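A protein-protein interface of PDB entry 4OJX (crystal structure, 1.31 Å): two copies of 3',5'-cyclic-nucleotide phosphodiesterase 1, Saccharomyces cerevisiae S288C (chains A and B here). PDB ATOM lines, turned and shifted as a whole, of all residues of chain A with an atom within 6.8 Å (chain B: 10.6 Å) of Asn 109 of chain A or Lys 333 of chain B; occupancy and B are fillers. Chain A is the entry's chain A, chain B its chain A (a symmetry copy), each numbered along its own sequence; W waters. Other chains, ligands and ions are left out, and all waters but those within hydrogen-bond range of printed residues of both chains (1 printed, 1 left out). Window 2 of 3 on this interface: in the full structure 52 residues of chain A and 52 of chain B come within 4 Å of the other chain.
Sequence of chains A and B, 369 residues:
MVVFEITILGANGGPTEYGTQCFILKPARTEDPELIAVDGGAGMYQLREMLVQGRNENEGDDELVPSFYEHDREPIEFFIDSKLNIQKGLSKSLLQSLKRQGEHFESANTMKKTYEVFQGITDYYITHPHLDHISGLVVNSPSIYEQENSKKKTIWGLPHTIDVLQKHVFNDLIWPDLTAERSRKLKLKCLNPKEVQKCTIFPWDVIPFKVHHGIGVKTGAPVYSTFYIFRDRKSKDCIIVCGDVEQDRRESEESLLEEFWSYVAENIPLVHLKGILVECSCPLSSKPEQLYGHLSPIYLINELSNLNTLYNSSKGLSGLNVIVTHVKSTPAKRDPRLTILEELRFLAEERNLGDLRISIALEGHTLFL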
ATOM      1  N   LEU A  51      -7.954  10.527  12.031  1.00  0.00           N
ATOM      2  CA  LEU A  51      -7.156  10.651  13.246  1.00  0.00           C
ATOM      3  C   LEU A  51      -7.433   9.470  14.197  1.00  0.00           C
ATOM      4  O   LEU A  51      -6.496   8.844  14.703  1.00  0.00           O
ATOM      5  CB  LEU A  51      -7.366  12.023  13.914  1.00  0.00           C
ATOM      6  CG  LEU A  51      -6.730  13.234  13.200  1.00  0.00           C
ATOM      7  CD1 LEU A  51      -7.353  14.549  13.652  1.00  0.00           C
ATOM      8  CD2 LEU A  51      -5.222  13.270  13.418  1.00  0.00           C
ATOM      9  N   HIS A 104       1.847  18.642  24.090  1.00  0.00           N
ATOM     10  CA  HIS A 104       0.642  19.297  23.560  1.00  0.00           C
ATOM     11  C   HIS A 104      -0.157  18.379  22.676  1.00  0.00           C
ATOM     12  O   HIS A 104      -1.374  18.262  22.845  1.00  0.00           O
ATOM     13  CB  HIS A 104       0.995  20.584  22.818  1.00  0.00           C
ATOM     14  CG  HIS A 104      -0.201  21.297  22.228  1.00  0.00           C
ATOM     15  ND1 HIS A 104      -0.852  22.277  22.880  1.00  0.00           N
ATOM     16  CD2 HIS A 104      -0.855  21.135  21.007  1.00  0.00           C
ATOM     17  CE1 HIS A 104      -1.870  22.723  22.119  1.00  0.00           C
ATOM     18  NE2 HIS A 104      -1.870  22.022  20.972  1.00  0.00           N
ATOM     19  N   PHE A 105       0.519  17.728  21.730  1.00  0.00           N
ATOM     20  CA  PHE A 105      -0.099  16.723  20.859  1.00  0.00           C
ATOM     21  C   PHE A 105      -0.810  15.641  21.667  1.00  0.00           C
ATOM     22  O   PHE A 105      -1.990  15.371  21.440  1.00  0.00           O
ATOM     23  CB  PHE A 105       0.948  16.082  19.933  1.00  0.00           C
ATOM     24  CG  PHE A 105       0.408  14.964  19.074  1.00  0.00           C
ATOM     25  CD1 PHE A 105      -0.349  15.241  17.940  1.00  0.00           C
ATOM     26  CD2 PHE A 105       0.661  13.631  19.399  1.00  0.00           C
ATOM     27  CE1 PHE A 105      -0.842  14.216  17.144  1.00  0.00           C
ATOM     28  CE2 PHE A 105       0.165  12.601  18.610  1.00  0.00           C
ATOM     29  CZ  PHE A 105      -0.587  12.895  17.479  1.00  0.00           C
ATOM     30  N   GLU A 106      -0.073  15.037  22.601  1.00  0.00           N
ATOM     31  CA  GLU A 106      -0.566  13.949  23.456  1.00  0.00           C
ATOM     32  C   GLU A 106      -1.800  14.333  24.246  1.00  0.00           C
ATOM     33  O   GLU A 106      -2.705  13.515  24.427  1.00  0.00           O
ATOM     34  CB  GLU A 106       0.503  13.532  24.472  1.00  0.00           C
ATOM     35  CG  GLU A 106       1.789  13.013  23.878  1.00  0.00           C
ATOM     36  CD  GLU A 106       2.764  12.538  24.938  1.00  0.00           C
ATOM     37  OE1 GLU A 106       3.810  12.003  24.552  1.00  0.00           O
ATOM     38  OE2 GLU A 106       2.511  12.698  26.156  1.00  0.00           O
ATOM     39  N   SER A 107      -1.803  15.563  24.746  1.00  0.00           N
ATOM     40  CA  SER A 107      -2.870  16.037  25.618  1.00  0.00           C
ATOM     41  C   SER A 107      -4.068  16.618  24.866  1.00  0.00           C
ATOM     42  O   SER A 107      -5.133  16.794  25.455  1.00  0.00           O
ATOM     43  CB  SER A 107      -2.318  17.046  26.619  1.00  0.00           C
ATOM     44  OG  SER A 107      -1.265  16.462  27.366  1.00  0.00           O
ATOM     45  N   ALA A 108      -3.896  16.919  23.577  1.00  0.00           N
ATOM     46  CA  ALA A 108      -4.992  17.411  22.743  1.00  0.00           C
ATOM     47  C   ALA A 108      -5.944  16.272  22.438  1.00  0.00           C
ATOM     48  O   ALA A 108      -5.535  15.227  21.937  1.00  0.00           O
ATOM     49  CB  ALA A 108      -4.448  18.003  21.452  1.00  0.00           C
ATOM     50  N   ASN A 109      -7.227  16.466  22.725  1.00  0.00           N
ATOM     51  CA  ASN A 109      -8.195  15.433  22.382  1.00  0.00           C
ATOM     52  C   ASN A 109      -8.426  15.356  20.866  1.00  0.00           C
ATOM     53  O   ASN A 109      -7.894  16.169  20.103  1.00  0.00           O
ATOM     54  CB  ASN A 109      -9.494  15.577  23.192  1.00  0.00           C
ATOM     55  CG  ASN A 109     -10.234  16.876  22.920  1.00  0.00           C
ATOM     56  OD1 ASN A 109     -10.304  17.349  21.783  1.00  0.00           O
ATOM     57  ND2 ASN A 109     -10.853  17.428  23.961  1.00  0.00           N
ATOM     58  N   THR A 110      -9.172  14.347  20.434  1.00  0.00           N
ATOM     59  CA  THR A 110      -9.371  14.130  19.007  1.00  0.00           C
ATOM     60  C   THR A 110     -10.024  15.338  18.335  1.00  0.00           C
ATOM     61  O   THR A 110      -9.620  15.726  17.242  1.00  0.00           O
ATOM     62  CB  THR A 110     -10.167  12.847  18.762  1.00  0.00           C
ATOM     63  OG1 THR A 110      -9.419  11.749  19.294  1.00  0.00           O
ATOM     64  CG2 THR A 110     -10.379  12.625  17.282  1.00  0.00           C
ATOM     65  N   MET A 111     -10.998  15.951  19.007  1.00  0.00           N
ATOM     66  CA  MET A 111     -11.640  17.142  18.468  1.00  0.00           C
ATOM     67  C   MET A 111     -10.652  18.286  18.275  1.00  0.00           C
ATOM     68  O   MET A 111     -10.654  18.948  17.239  1.00  0.00           O
ATOM     69  CB  MET A 111     -12.791  17.591  19.370  1.00  0.00           C
ATOM     70  CG  MET A 111     -13.724  18.610  18.728  1.00  0.00           C
ATOM     71  SD  MET A 111     -14.709  17.940  17.367  1.00  0.00           S
ATOM     72  CE  MET A 111     -13.909  18.617  15.922  1.00  0.00           C
ATOM     73  N   LYS A 112      -9.811  18.515  19.283  1.00  0.00           N
ATOM     74  CA  LYS A 112      -8.812  19.564  19.210  1.00  0.00           C
ATOM     75  C   LYS A 112      -7.820  19.302  18.080  1.00  0.00           C
ATOM     76  O   LYS A 112      -7.476  20.218  17.334  1.00  0.00           O
ATOM     77  CB  LYS A 112      -8.083  19.714  20.547  1.00  0.00           C
ATOM     78  CG  LYS A 112      -7.025  20.809  20.584  1.00  0.00           C
ATOM     79  CD  LYS A 112      -7.633  22.187  20.377  1.00  0.00           C
ATOM     80  CE  LYS A 112      -6.589  23.286  20.482  1.00  0.00           C
ATOM     81  NZ  LYS A 112      -7.199  24.618  20.215  1.00  0.00           N
ATOM     82  N   LYS A 113      -7.364  18.057  17.950  1.00  0.00           N
ATOM     83  CA  LYS A 113      -6.461  17.701  16.851  1.00  0.00           C
ATOM     84  C   LYS A 113      -7.107  17.981  15.500  1.00  0.00           C
ATOM     85  O   LYS A 113      -6.443  18.432  14.569  1.00  0.00           O
ATOM     86  CB  LYS A 113      -6.055  16.229  16.933  1.00  0.00           C
ATOM     87  CG  LYS A 113      -5.122  15.858  18.082  1.00  0.00           C
ATOM     88  CD  LYS A 113      -4.676  14.409  17.927  1.00  0.00           C
ATOM     89  CE  LYS A 113      -3.788  13.917  19.061  1.00  0.00           C
ATOM     90  NZ  LYS A 113      -4.564  13.346  20.196  1.00  0.00           N
ATOM     91  N   THR A 114      -8.410  17.700  15.395  1.00  0.00           N
ATOM     92  CA  THR A 114      -9.155  17.925  14.164  1.00  0.00           C
ATOM     93  C   THR A 114      -9.152  19.406  13.802  1.00  0.00           C
ATOM     94  O   THR A 114      -8.857  19.773  12.661  1.00  0.00           O
ATOM     95  CB  THR A 114     -10.594  17.397  14.284  1.00  0.00           C
ATOM     96  OG1 THR A 114     -10.554  16.000  14.575  1.00  0.00           O
ATOM     97  CG2 THR A 114     -11.356  17.598  12.988  1.00  0.00           C
ATOM     98  N   SER B  67     -17.843  10.506  20.923  1.00  0.00           N
ATOM     99  CA  SER B  67     -17.689  11.759  21.645  1.00  0.00           C
ATOM    100  C   SER B  67     -16.537  12.586  21.074  1.00  0.00           C
ATOM    101  O   SER B  67     -16.756  13.663  20.515  1.00  0.00           O
ATOM    102  CB  SER B  67     -17.511  11.507  23.146  1.00  0.00           C
ATOM    103  OG  SER B  67     -17.149  12.694  23.815  1.00  0.00           O
ATOM    104  N   PHE B  68     -15.319  12.065  21.229  1.00  0.00           N
ATOM    105  CA  PHE B  68     -14.073  12.639  20.691  1.00  0.00           C
ATOM    106  C   PHE B  68     -13.441  13.740  21.536  1.00  0.00           C
ATOM    107  O   PHE B  68     -12.594  14.488  21.055  1.00  0.00           O
ATOM    108  CB  PHE B  68     -14.197  13.038  19.210  1.00  0.00           C
ATOM    109  CG  PHE B  68     -14.704  11.926  18.333  1.00  0.00           C
ATOM    110  CD1 PHE B  68     -13.976  10.747  18.175  1.00  0.00           C
ATOM    111  CD2 PHE B  68     -15.928  12.046  17.687  1.00  0.00           C
ATOM    112  CE1 PHE B  68     -14.460   9.719  17.378  1.00  0.00           C
ATOM    113  CE2 PHE B  68     -16.411  11.025  16.879  1.00  0.00           C
ATOM    114  CZ  PHE B  68     -15.679   9.861  16.727  1.00  0.00           C
ATOM    115  N   TYR B  69     -13.838  13.817  22.805  1.00  0.00           N
ATOM    116  CA  TYR B  69     -13.273  14.783  23.732  1.00  0.00           C
ATOM    117  C   TYR B  69     -12.424  14.034  24.755  1.00  0.00           C
ATOM    118  O   TYR B  69     -11.421  13.428  24.381  1.00  0.00           O
ATOM    119  CB  TYR B  69     -14.377  15.648  24.340  1.00  0.00           C
ATOM    120  CG  TYR B  69     -15.041  16.522  23.298  1.00  0.00           C
ATOM    121  CD1 TYR B  69     -16.059  16.021  22.482  1.00  0.00           C
ATOM    122  CD2 TYR B  69     -14.631  17.835  23.107  1.00  0.00           C
ATOM    123  CE1 TYR B  69     -16.667  16.813  21.515  1.00  0.00           C
ATOM    124  CE2 TYR B  69     -15.230  18.639  22.142  1.00  0.00           C
ATOM    125  CZ  TYR B  69     -16.249  18.119  21.354  1.00  0.00           C
ATOM    126  OH  TYR B  69     -16.857  18.918  20.397  1.00  0.00           O
ATOM    127  N   GLU B  70     -12.808  14.042  26.022  1.00  0.00           N
ATOM    128  CA  GLU B  70     -12.052  13.273  27.019  1.00  0.00           C
ATOM    129  C   GLU B  70     -11.845  11.817  26.599  1.00  0.00           C
ATOM    130  O   GLU B  70     -10.785  11.237  26.849  1.00  0.00           O
ATOM    131  CB  GLU B  70     -12.722  13.379  28.383  1.00  0.00           C
ATOM    132  CG  GLU B  70     -12.594  14.778  28.965  1.00  0.00           C
ATOM    133  CD  GLU B  70     -13.511  15.023  30.138  1.00  0.00           C
ATOM    134  OE1 GLU B  70     -14.710  14.691  30.054  1.00  0.00           O
ATOM    135  OE2 GLU B  70     -13.026  15.569  31.156  1.00  0.00           O
ATOM    136  N   HIS B  71     -12.856  11.227  25.968  1.00  0.00           N
ATOM    137  CA  HIS B  71     -12.733   9.911  25.359  1.00  0.00           C
ATOM    138  C   HIS B  71     -13.331   9.943  23.990  1.00  0.00           C
ATOM    139  O   HIS B  71     -14.253  10.716  23.716  1.00  0.00           O
ATOM    140  CB  HIS B  71     -13.453   8.848  26.175  1.00  0.00           C
ATOM    141  CG  HIS B  71     -13.001   8.776  27.603  1.00  0.00           C
ATOM    142  ND1 HIS B  71     -13.603   9.475  28.579  1.00  0.00           N
ATOM    143  CD2 HIS B  71     -11.960   8.074  28.197  1.00  0.00           C
ATOM    144  CE1 HIS B  71     -12.983   9.218  29.750  1.00  0.00           C
ATOM    145  NE2 HIS B  71     -11.980   8.366  29.508  1.00  0.00           N
ATOM    146  N   ASP B  72     -12.833   9.080  23.117  1.00  0.00           N
ATOM    147  CA  ASP B  72     -13.422   8.966  21.792  1.00  0.00           C
ATOM    148  C   ASP B  72     -14.843   8.379  21.848  1.00  0.00           C
ATOM    149  O   ASP B  72     -15.665   8.692  20.995  1.00  0.00           O
ATOM    150  CB  ASP B  72     -12.511   8.176  20.844  1.00  0.00           C
ATOM    151  CG  ASP B  72     -11.270   8.958  20.426  1.00  0.00           C
ATOM    152  OD1 ASP B  72     -11.238  10.207  20.530  1.00  0.00           O
ATOM    153  OD2 ASP B  72     -10.307   8.317  19.970  1.00  0.00           O
ATOM    154  N   ARG B  73     -15.132   7.546  22.845  1.00  0.00           N
ATOM    155  CA  ARG B  73     -16.475   7.023  23.071  1.00  0.00           C
ATOM    156  C   ARG B  73     -16.838   7.177  24.543  1.00  0.00           C
ATOM    157  O   ARG B  73     -15.972   7.045  25.411  1.00  0.00           O
ATOM    158  CB  ARG B  73     -16.566   5.553  22.655  1.00  0.00           C
ATOM    159  CG  ARG B  73     -16.313   5.293  21.177  1.00  0.00           C
ATOM    160  CD  ARG B  73     -16.134   3.805  20.912  1.00  0.00           C
ATOM    161  NE  ARG B  73     -17.406   3.087  20.945  1.00  0.00           N
ATOM    162  CZ  ARG B  73     -17.531   1.775  21.136  1.00  0.00           C
ATOM    163  NH1 ARG B  73     -16.460   1.012  21.328  1.00  0.00           N
ATOM    164  NH2 ARG B  73     -18.737   1.223  21.143  1.00  0.00           N
ATOM    165  N   GLU B  74     -18.109   7.459  24.823  1.00  0.00           N
ATOM    166  CA  GLU B  74     -18.598   7.675  26.183  1.00  0.00           C
ATOM    167  C   GLU B  74     -19.863   6.878  26.448  1.00  0.00           C
ATOM    168  O   GLU B  74     -20.670   6.676  25.539  1.00  0.00           O
ATOM    169  CB  GLU B  74     -18.927   9.148  26.412  1.00  0.00           C
ATOM    170  CG  GLU B  74     -17.740  10.087  26.473  1.00  0.00           C
ATOM    171  CD  GLU B  74     -16.894   9.937  27.730  1.00  0.00           C
ATOM    172  OE1 GLU B  74     -17.215   9.118  28.624  1.00  0.00           O
ATOM    173  OE2 GLU B  74     -15.879  10.640  27.804  1.00  0.00           O
ATOM    174  N   PRO B 283     -22.609  26.216  24.983  1.00  0.00           N
ATOM    175  CA  PRO B 283     -22.619  26.232  26.448  1.00  0.00           C
ATOM    176  C   PRO B 283     -22.663  27.666  26.967  1.00  0.00           C
ATOM    177  O   PRO B 283     -22.623  28.620  26.187  1.00  0.00           O
ATOM    178  CB  PRO B 283     -21.276  25.599  26.792  1.00  0.00           C
ATOM    179  CG  PRO B 283     -20.388  26.089  25.697  1.00  0.00           C
ATOM    180  CD  PRO B 283     -21.247  25.999  24.459  1.00  0.00           C
ATOM    181  N   SER B 285     -20.366  29.376  28.420  1.00  0.00           N
ATOM    182  CA  SER B 285     -19.118  30.119  28.179  1.00  0.00           C
ATOM    183  C   SER B 285     -19.181  30.940  26.886  1.00  0.00           C
ATOM    184  O   SER B 285     -18.339  31.811  26.651  1.00  0.00           O
ATOM    185  CB  SER B 285     -17.918  29.170  28.163  1.00  0.00           C
ATOM    186  OG  SER B 285     -18.047  28.211  27.127  1.00  0.00           O
ATOM    187  N   LYS B 287     -18.788  31.982  23.337  1.00  0.00           N
ATOM    188  CA  LYS B 287     -18.068  32.914  22.481  1.00  0.00           C
ATOM    189  C   LYS B 287     -19.078  33.467  21.472  1.00  0.00           C
ATOM    190  O   LYS B 287     -19.753  32.688  20.790  1.00  0.00           O
ATOM    191  CB  LYS B 287     -16.911  32.207  21.769  1.00  0.00           C
ATOM    192  CG  LYS B 287     -15.875  31.606  22.711  1.00  0.00           C
ATOM    193  CD  LYS B 287     -14.853  30.769  21.962  1.00  0.00           C
ATOM    194  CE  LYS B 287     -13.862  30.130  22.921  1.00  0.00           C
ATOM    195  NZ  LYS B 287     -12.899  29.241  22.213  1.00  0.00           N
ATOM    196  N   LYS B 328     -23.074  22.219  18.993  1.00  0.00           N
ATOM    197  CA  LYS B 328     -21.909  22.431  18.148  1.00  0.00           C
ATOM    198  C   LYS B 328     -20.648  21.803  18.735  1.00  0.00           C
ATOM    199  O   LYS B 328     -20.492  21.722  19.962  1.00  0.00           O
ATOM    200  CB  LYS B 328     -21.709  23.927  17.933  1.00  0.00           C
ATOM    201  CG  LYS B 328     -22.750  24.502  16.987  1.00  0.00           C
ATOM    202  CD  LYS B 328     -22.575  25.991  16.759  1.00  0.00           C
ATOM    203  CE  LYS B 328     -23.626  26.541  15.805  1.00  0.00           C
ATOM    204  NZ  LYS B 328     -23.529  26.003  14.412  1.00  0.00           N
ATOM    205  N   SER B 329     -19.731  21.369  17.873  1.00  0.00           N
ATOM    206  CA  SER B 329     -18.373  21.042  18.340  1.00  0.00           C
ATOM    207  C   SER B 329     -17.692  22.317  18.785  1.00  0.00           C
ATOM    208  O   SER B 329     -18.049  23.428  18.358  1.00  0.00           O
ATOM    209  CB  SER B 329     -17.517  20.410  17.251  1.00  0.00           C
ATOM    210  OG  SER B 329     -18.091  19.212  16.813  1.00  0.00           O
ATOM    211  N   THR B 330     -16.691  22.155  19.624  1.00  0.00           N
ATOM    212  CA  THR B 330     -15.882  23.259  20.066  1.00  0.00           C
ATOM    213  C   THR B 330     -14.540  22.636  20.427  1.00  0.00           C
ATOM    214  O   THR B 330     -14.487  21.454  20.784  1.00  0.00           O
ATOM    215  CB  THR B 330     -16.545  23.968  21.269  1.00  0.00           C
ATOM    216  OG1 THR B 330     -15.765  25.105  21.653  1.00  0.00           O
ATOM    217  CG2 THR B 330     -16.704  23.019  22.453  1.00  0.00           C
ATOM    218  N   PRO B 331     -13.439  23.398  20.301  1.00  0.00           N
ATOM    219  CA  PRO B 331     -12.146  22.837  20.706  1.00  0.00           C
ATOM    220  C   PRO B 331     -11.953  22.936  22.221  1.00  0.00           C
ATOM    221  O   PRO B 331     -11.012  23.574  22.695  1.00  0.00           O
ATOM    222  CB  PRO B 331     -11.130  23.696  19.939  1.00  0.00           C
ATOM    223  CG  PRO B 331     -11.831  24.978  19.664  1.00  0.00           C
ATOM    224  CD  PRO B 331     -13.302  24.691  19.602  1.00  0.00           C
ATOM    225  N   ALA B 332     -12.887  22.335  22.956  1.00  0.00           N
ATOM    226  CA  ALA B 332     -12.895  22.327  24.413  1.00  0.00           C
ATOM    227  C   ALA B 332     -12.387  20.995  24.947  1.00  0.00           C
ATOM    228  O   ALA B 332     -12.327  19.995  24.219  1.00  0.00           O
ATOM    229  CB  ALA B 332     -14.293  22.603  24.939  1.00  0.00           C
ATOM    230  N   LYS B 333     -12.022  20.984  26.226  1.00  0.00           N
ATOM    231  CA  LYS B 333     -11.516  19.766  26.852  1.00  0.00           C
ATOM    232  C   LYS B 333     -12.617  18.724  27.043  1.00  0.00           C
ATOM    233  O   LYS B 333     -12.368  17.533  26.901  1.00  0.00           O
ATOM    234  CB  LYS B 333     -10.836  20.072  28.188  1.00  0.00           C
ATOM    235  CG  LYS B 333      -9.565  20.897  28.046  1.00  0.00           C
ATOM    236  CD  LYS B 333      -8.867  21.107  29.381  1.00  0.00           C
ATOM    237  CE  LYS B 333      -7.543  21.832  29.194  1.00  0.00           C
ATOM    238  NZ  LYS B 333      -6.849  22.067  30.490  1.00  0.00           N
ATOM    239  N   ARG B 334     -13.831  19.184  27.340  1.00  0.00           N
ATOM    240  CA  ARG B 334     -14.953  18.300  27.647  1.00  0.00           C
ATOM    241  C   ARG B 334     -16.038  18.403  26.579  1.00  0.00           C
ATOM    242  O   ARG B 334     -16.291  19.475  26.034  1.00  0.00           O
ATOM    243  CB  ARG B 334     -15.521  18.631  29.030  1.00  0.00           C
ATOM    244  CG  ARG B 334     -16.564  17.654  29.557  1.00  0.00           C
ATOM    245  CD  ARG B 334     -16.495  17.560  31.076  1.00  0.00           C
ATOM    246  NE  ARG B 334     -17.440  16.585  31.624  1.00  0.00           N
ATOM    247  CZ  ARG B 334     -18.639  16.885  32.104  1.00  0.00           C
ATOM    248  NH1 ARG B 334     -19.068  18.143  32.109  1.00  0.00           N
ATOM    249  NH2 ARG B 334     -19.413  15.923  32.585  1.00  0.00           N
ATOM    250  N   ASP B 335     -16.668  17.275  26.294  1.00  0.00           N
ATOM    251  CA  ASP B 335     -17.769  17.201  25.342  1.00  0.00           C
ATOM    252  C   ASP B 335     -18.818  18.256  25.690  1.00  0.00           C
ATOM    253  O   ASP B 335     -19.372  18.243  26.792  1.00  0.00           O
ATOM    254  CB  ASP B 335     -18.348  15.789  25.419  1.00  0.00           C
ATOM    255  CG  ASP B 335     -19.309  15.448  24.284  1.00  0.00           C
ATOM    256  OD1 ASP B 335     -20.151  16.293  23.892  1.00  0.00           O
ATOM    257  OD2 ASP B 335     -19.231  14.288  23.821  1.00  0.00           O
ATOM    258  N   PRO B 336     -19.097  19.187  24.756  1.00  0.00           N
ATOM    259  CA  PRO B 336     -20.028  20.264  25.097  1.00  0.00           C
ATOM    260  C   PRO B 336     -21.441  19.760  25.341  1.00  0.00           C
ATOM    261  O   PRO B 336     -22.206  20.431  26.016  1.00  0.00           O
ATOM    262  CB  PRO B 336     -19.985  21.185  23.868  1.00  0.00           C
ATOM    263  CG  PRO B 336     -19.499  20.311  22.764  1.00  0.00           C
ATOM    264  CD  PRO B 336     -18.525  19.367  23.409  1.00  0.00           C
ATOM    265  N   ARG B 337     -21.790  18.592  24.815  1.00  0.00           N
ATOM    266  CA  ARG B 337     -23.095  18.023  25.131  1.00  0.00           C
ATOM    267  C   ARG B 337     -23.233  17.736  26.624  1.00  0.00           C
ATOM    268  O   ARG B 337     -24.294  17.961  27.211  1.00  0.00           O
ATOM    269  CB  ARG B 337     -23.331  16.759  24.322  1.00  0.00           C
ATOM    270  CG  ARG B 337     -23.401  17.031  22.828  1.00  0.00           C
ATOM    271  CD  ARG B 337     -23.452  15.763  22.011  1.00  0.00           C
ATOM    272  NE  ARG B 337     -22.265  14.948  22.228  1.00  0.00           N
ATOM    273  CZ  ARG B 337     -22.117  13.706  21.784  1.00  0.00           C
ATOM    274  NH1 ARG B 337     -23.079  13.135  21.058  1.00  0.00           N
ATOM    275  NH2 ARG B 337     -21.001  13.036  22.049  1.00  0.00           N
ATOM    276  N   LEU B 338     -22.145  17.268  27.242  1.00  0.00           N
ATOM    277  CA  LEU B 338     -22.149  17.016  28.682  1.00  0.00           C
ATOM    278  C   LEU B 338     -22.196  18.318  29.474  1.00  0.00           C
ATOM    279  O   LEU B 338     -22.981  18.454  30.415  1.00  0.00           O
ATOM    280  CB  LEU B 338     -20.956  16.150  29.080  1.00  0.00           C
ATOM    281  CG  LEU B 338     -20.916  14.759  28.433  1.00  0.00           C
ATOM    282  CD1 LEU B 338     -19.624  14.038  28.781  1.00  0.00           C
ATOM    283  CD2 LEU B 338     -22.131  13.934  28.837  1.00  0.00           C
ATOM    284  N   THR B 339     -21.390  19.296  29.061  1.00  0.00           N
ATOM    285  CA  THR B 339     -21.393  20.603  29.699  1.00  0.00           C
ATOM    286  C   THR B 339     -22.789  21.225  29.655  1.00  0.00           C
ATOM    287  O   THR B 339     -23.323  21.687  30.672  1.00  0.00           O
ATOM    288  CB  THR B 339     -20.376  21.523  29.010  1.00  0.00           C
ATOM    289  OG1 THR B 339     -19.082  20.916  29.088  1.00  0.00           O
ATOM    290  CG2 THR B 339     -20.350  22.906  29.641  1.00  0.00           C
HETATM  291  O   HOH W   1      -9.830  16.668  26.645  1.00  0.00           O
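ND2 of Asn 109 of chain A sits at hydrogen-bond distance from O of Ala 332 of chain B, 3.0 Å away. ND2 of Asn 109 of chain A sits at hydrogen-bond distance from O of Lys 333 of chain B (3.3 Å). The backbone NH (N) of Thr 110 of chain A is in hydrogen-bond range of the backbone carbonyl oxygen (O) of Phe 68 of chain B (3.5 Å). The side-chain hydroxyl (OG1) of Thr 110 of chain A sits at hydrogen-bond distance from the side-chain carboxylate (OD1) of Asp 72 of chain B, at 2.7 Å. O of Phe 68 of chain B sits at hydrogen-bond distance from N of Met 111 of chain A (3.0 Å). The side-chain hydroxyl (OG) of Ser 329 of chain B is in hydrogen-bond range of the side-chain sulfur (SD) of Met 111 of chain A, 3.7 Å away.
OD1 of Asn 109 of chain A lies within hydrogen-bond range of N of Met 111 of chain A, at 3.2 Å. The side-chain amide oxygen of Asn 109 of chain A lies within hydrogen-bond range of the backbone NH of Lys 112 of chain A (2.8 Å). The backbone carbonyl oxygen of Thr 110 of chain A lies within hydrogen-bond range of the side-chain hydroxyl of Thr 114 of chain A, 2.8 Å away. The backbone NH (N) of Ser 67 of chain B lies within hydrogen-bond range of the backbone carbonyl oxygen (O) of Asp 72 of chain B (2.8 Å). The side-chain hydroxyl (OH) of Tyr 69 of chain B lies within hydrogen-bond range of the backbone NH (N) of Thr 330 of chain B (3.3 Å).
Among the printed residues, pairs that only touch across the chains: Asn 109 of chain A with Phe 68 of chain B, Asn 109 of chain A with Tyr 69 of chain B, Met 111 of chain A with Tyr 69 of chain B, Met 111 of chain A with Thr 330 of chain B and Lys 112 of chain A with Pro 331 of chain B.
Ala 108 of chain A touches none of the printed residues of chain B. Of chain B, only Phe 68 (3.7 Å), Tyr 69 (3.1 Å), Ala 332 (3.0 Å) and Lys 333 (3.3 Å) come within 4 Å of Asn 109 of chain A. Thr 110 of chain A touches just these residues of chain B: Phe 68 and Asp 72. Of the printed residues of chain B, Lys 112 of chain A touches Pro 331. No residue of chain B comes within 4 Å of Lys 113 of chain A. Of the printed residues of chain A, Thr 330 of chain B touches Met 111 (3.6 Å). Printed residues of chain A within 4 Å of Pro 331 of chain B: Lys 112 (3.8 Å). Of chain A, only Asn 109 (3.3 Å) comes within 4 Å of Lys 333 of chain B. The nearest residue of chain B that does not touch Asn 109 of chain A is Glu 70 of chain B (4.4 Å). The nearest residue of chain A that does not touch Lys 333 of chain B is Ser 107 of chain A (6.6 Å). The nearest printed residue of chain B that does not touch Lys 112 of chain A is Phe 68 of chain B (5.2 Å).
Of the 23 printed residues of chain B, 8 touch a printed residue of chain A. Hydrophobic or aromatic side chains of chain B within 4 Å of the printed part of chain A: Tyr 69 and Pro 331.
No position is printed for both chains.
Water W1 lies within hydrogen-bond range of the backbone carbonyl oxygen of Lys 333 of chain B (2.7 Å) and the side-chain amide nitrogen of Asn 109 of chain A (3.0 Å).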
